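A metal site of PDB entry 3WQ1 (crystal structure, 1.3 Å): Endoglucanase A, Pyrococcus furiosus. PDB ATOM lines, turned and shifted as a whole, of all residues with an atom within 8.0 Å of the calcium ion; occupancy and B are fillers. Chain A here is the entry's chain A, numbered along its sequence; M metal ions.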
ATOM      1  N   ILE A  67       3.961 -13.030   4.039  1.00  0.00           N
ATOM      2  CA  ILE A  67       3.495 -13.344   5.382  1.00  0.00           C
ATOM      3  C   ILE A  67       2.136 -13.964   5.198  1.00  0.00           C
ATOM      4  O   ILE A  67       1.194 -13.360   4.699  1.00  0.00           O
ATOM      5  CB  ILE A  67       3.391 -12.118   6.274  1.00  0.00           C
ATOM      6  CG1 ILE A  67       4.841 -11.578   6.543  1.00  0.00           C
ATOM      7  CG2 ILE A  67       2.654 -12.440   7.574  1.00  0.00           C
ATOM      8  CD1 ILE A  67       4.827 -10.216   7.205  1.00  0.00           C
ATOM      9  N   ASP A  68       1.998 -15.275   5.545  1.00  0.00           N
ATOM     10  CA  ASP A  68       0.798 -16.054   5.312  1.00  0.00           C
ATOM     11  C   ASP A  68       0.555 -16.882   6.592  1.00  0.00           C
ATOM     12  O   ASP A  68       0.827 -18.095   6.616  1.00  0.00           O
ATOM     13  CB  ASP A  68       1.000 -16.942   4.070  1.00  0.00           C
ATOM     14  CG  ASP A  68      -0.241 -17.752   3.699  1.00  0.00           C
ATOM     15  OD1 ASP A  68      -1.343 -17.451   4.169  1.00  0.00           O
ATOM     16  OD2 ASP A  68      -0.062 -18.665   2.856  1.00  0.00           O
ATOM     17  N   LYS A  69      -0.021 -16.226   7.580  1.00  0.00           N
ATOM     18  CA  LYS A  69      -0.080 -16.829   8.903  1.00  0.00           C
ATOM     19  C   LYS A  69      -0.998 -18.064   8.971  1.00  0.00           C
ATOM     20  O   LYS A  69      -0.721 -18.972   9.764  1.00  0.00           O
ATOM     21  CB  LYS A  69      -0.588 -15.748   9.923  1.00  0.00           C
ATOM     22  CG  LYS A  69      -0.482 -16.171  11.411  1.00  0.00           C
ATOM     23  CD  LYS A  69      -0.408 -14.936  12.360  1.00  0.00           C
ATOM     24  CE  LYS A  69       0.755 -13.898  12.177  1.00  0.00           C
ATOM     25  NZ  LYS A  69       0.677 -12.470  11.558  1.00  0.00           N
ATOM     26  N   ASP A  70      -2.039 -18.085   8.166  1.00  0.00           N
ATOM     27  CA  ASP A  70      -2.992 -19.222   8.100  1.00  0.00           C
ATOM     28  C   ASP A  70      -2.547 -20.218   7.046  1.00  0.00           C
ATOM     29  O   ASP A  70      -3.229 -21.238   6.930  1.00  0.00           O
ATOM     30  CB  ASP A  70      -4.469 -18.677   7.983  1.00  0.00           C
ATOM     31  CG  ASP A  70      -4.738 -17.985   6.686  1.00  0.00           C
ATOM     32  OD1 ASP A  70      -3.763 -17.596   5.982  1.00  0.00           O
ATOM     33  OD2 ASP A  70      -5.947 -17.788   6.336  1.00  0.00           O
ATOM     34  N   GLY A  71      -1.397 -20.013   6.376  1.00  0.00           N
ATOM     35  CA  GLY A  71      -0.897 -20.967   5.398  1.00  0.00           C
ATOM     36  C   GLY A  71      -1.908 -21.271   4.322  1.00  0.00           C
ATOM     37  O   GLY A  71      -1.934 -22.391   3.768  1.00  0.00           O
ATOM     38  N   ASP A  72      -2.722 -20.271   3.914  1.00  0.00           N
ATOM     39  CA  ASP A  72      -3.783 -20.538   2.909  1.00  0.00           C
ATOM     40  C   ASP A  72      -3.345 -20.155   1.496  1.00  0.00           C
ATOM     41  O   ASP A  72      -4.194 -20.248   0.576  1.00  0.00           O
ATOM     42  CB  ASP A  72      -5.133 -19.954   3.335  1.00  0.00           C
ATOM     43  CG  ASP A  72      -5.208 -18.436   3.073  1.00  0.00           C
ATOM     44  OD1 ASP A  72      -4.180 -17.734   2.883  1.00  0.00           O
ATOM     45  OD2 ASP A  72      -6.364 -17.912   3.081  1.00  0.00           O
ATOM     46  N   GLY A  73      -2.101 -19.752   1.268  1.00  0.00           N
ATOM     47  CA  GLY A  73      -1.678 -19.414  -0.097  1.00  0.00           C
ATOM     48  C   GLY A  73      -2.039 -17.996  -0.561  1.00  0.00           C
ATOM     49  O   GLY A  73      -1.699 -17.672  -1.688  1.00  0.00           O
ATOM     50  N   ASN A  74      -2.646 -17.224   0.319  1.00  0.00           N
ATOM     51  CA  ASN A  74      -2.929 -15.825   0.012  1.00  0.00           C
ATOM     52  C   ASN A  74      -2.257 -14.994   1.139  1.00  0.00           C
ATOM     53  O   ASN A  74      -2.724 -15.034   2.306  1.00  0.00           O
ATOM     54  CB  ASN A  74      -4.427 -15.593  -0.028  1.00  0.00           C
ATOM     55  CG  ASN A  74      -4.781 -14.206  -0.558  1.00  0.00           C
ATOM     56  OD1 ASN A  74      -3.880 -13.437  -1.032  1.00  0.00           O
ATOM     57  ND2 ASN A  74      -6.082 -13.893  -0.498  1.00  0.00           N
ATOM     58  N   PRO A  75      -1.182 -14.296   0.822  1.00  0.00           N
ATOM     59  CA  PRO A  75      -0.488 -13.604   1.938  1.00  0.00           C
ATOM     60  C   PRO A  75      -1.323 -12.479   2.512  1.00  0.00           C
ATOM     61  O   PRO A  75      -2.075 -11.821   1.776  1.00  0.00           O
ATOM     62  CB  PRO A  75       0.795 -13.054   1.268  1.00  0.00           C
ATOM     63  CG  PRO A  75       0.957 -13.905   0.005  1.00  0.00           C
ATOM     64  CD  PRO A  75      -0.451 -14.172  -0.422  1.00  0.00           C
ATOM     65  N   GLU A  76      -1.224 -12.216   3.825  1.00  0.00           N
ATOM     66  CA  GLU A  76      -1.813 -11.045   4.470  1.00  0.00           C
ATOM     67  C   GLU A  76      -0.973  -9.790   4.157  1.00  0.00           C
ATOM     68  O   GLU A  76      -1.536  -8.709   4.062  1.00  0.00           O
ATOM     69  CB  GLU A  76      -1.933 -11.225   5.991  1.00  0.00           C
ATOM     70  CG  GLU A  76      -2.810 -12.394   6.385  1.00  0.00           C
ATOM     71  CD  GLU A  76      -2.012 -13.693   6.462  1.00  0.00           C
ATOM     72  OE1 GLU A  76      -1.007 -13.689   7.202  1.00  0.00           O
ATOM     73  OE2 GLU A  76      -2.335 -14.725   5.814  1.00  0.00           O
ATOM     74  N   PHE A  77       0.343  -9.980   4.055  1.00  0.00           N
ATOM     75  CA  PHE A  77       1.249  -8.901   3.735  1.00  0.00           C
ATOM     76  C   PHE A  77       2.424  -9.500   2.994  1.00  0.00           C
ATOM     77  O   PHE A  77       2.604 -10.756   3.025  1.00  0.00           O
ATOM     78  CB  PHE A  77       1.775  -8.202   5.007  1.00  0.00           C
ATOM     79  CG  PHE A  77       0.758  -7.445   5.776  1.00  0.00           C
ATOM     80  CD1 PHE A  77       0.332  -6.208   5.361  1.00  0.00           C
ATOM     81  CD2 PHE A  77       0.129  -8.036   6.889  1.00  0.00           C
ATOM     82  CE1 PHE A  77      -0.692  -5.536   6.047  1.00  0.00           C
ATOM     83  CE2 PHE A  77      -0.854  -7.393   7.574  1.00  0.00           C
ATOM     84  CZ  PHE A  77      -1.271  -6.156   7.154  1.00  0.00           C
ATOM     85  N   THR A 141      -3.228 -10.363  -0.645  1.00  0.00           N
ATOM     86  CA  THR A 141      -4.614  -9.955  -0.774  1.00  0.00           C
ATOM     87  C   THR A 141      -5.498 -10.556   0.287  1.00  0.00           C
ATOM     88  O   THR A 141      -6.725 -10.463   0.169  1.00  0.00           O
ATOM     89  CB  THR A 141      -5.188 -10.165  -2.187  1.00  0.00           C
ATOM     90  OG1 THR A 141      -5.321 -11.527  -2.410  1.00  0.00           O
ATOM     91  CG2 THR A 141      -4.360  -9.419  -3.236  1.00  0.00           C
ATOM     92  N   ASP A 142      -4.910 -11.116   1.361  1.00  0.00           N
ATOM     93  CA  ASP A 142      -5.750 -11.706   2.459  1.00  0.00           C
ATOM     94  C   ASP A 142      -5.989 -10.604   3.468  1.00  0.00           C
ATOM     95  O   ASP A 142      -5.188 -10.489   4.401  1.00  0.00           O
ATOM     96  CB  ASP A 142      -5.009 -12.924   2.953  1.00  0.00           C
ATOM     97  CG  ASP A 142      -5.832 -13.760   3.944  1.00  0.00           C
ATOM     98  OD1 ASP A 142      -6.931 -13.344   4.328  1.00  0.00           O
ATOM     99  OD2 ASP A 142      -5.274 -14.835   4.313  1.00  0.00           O
ATOM    100  N   GLY A 143      -6.996  -9.786   3.277  1.00  0.00           N
ATOM    101  CA  GLY A 143      -7.321  -8.658   4.158  1.00  0.00           C
ATOM    102  C   GLY A 143      -8.638  -8.074   3.793  1.00  0.00           C
ATOM    103  O   GLY A 143      -9.280  -8.491   2.802  1.00  0.00           O
HETATM  104 CA    CA M   1      -3.302 -16.098   4.286  1.00  0.00          CA
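Of the 14 residues printed, 6 come within 4 Å of the calcium ion. The nearest printed residue that does not touch the calcium ion is Pro 75 (4.4 Å).
The side-chain carboxylate (OE2) of Glu 76 is bound to the calcium ion, 2.3 Å away. The calcium ion is bound by the side-chain carboxylate (OD1) of Asp 70, 2.3 Å away. The calcium ion is bound by the backbone carbonyl oxygen (O) of Asn 74 (2.3 Å). OD1 of Asp 72 is bound to the calcium ion (2.3 Å). OD2 of Asp 142 binds the calcium ion, 2.3 Å away. The side-chain carboxylate (OD1) of Asp 68 is bound to the calcium ion (2.4 Å). The calcium ion has six donor atoms within binding distance.
The side-chain carboxylate of Glu 76 is in hydrogen-bond range of the backbone NH of Lys 69 (2.7 Å). N of Glu 76 sits at hydrogen-bond distance from O of Ile 67 (2.8 Å). The side-chain hydroxyl of Thr 141 sits at hydrogen-bond distance from the side-chain amide oxygen of Asn 74, at 2.8 Å. The backbone carbonyl oxygen (O) of Pro 75 lies within hydrogen-bond range of the backbone NH (N) of Asp 142. The backbone NH of Gly 71 sits close to the side-chain carboxylate of Asp 68 (3.4 Å). N of Gly 73 lies within hydrogen-bond range of OD2 of Asp 68 (2.8 Å).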
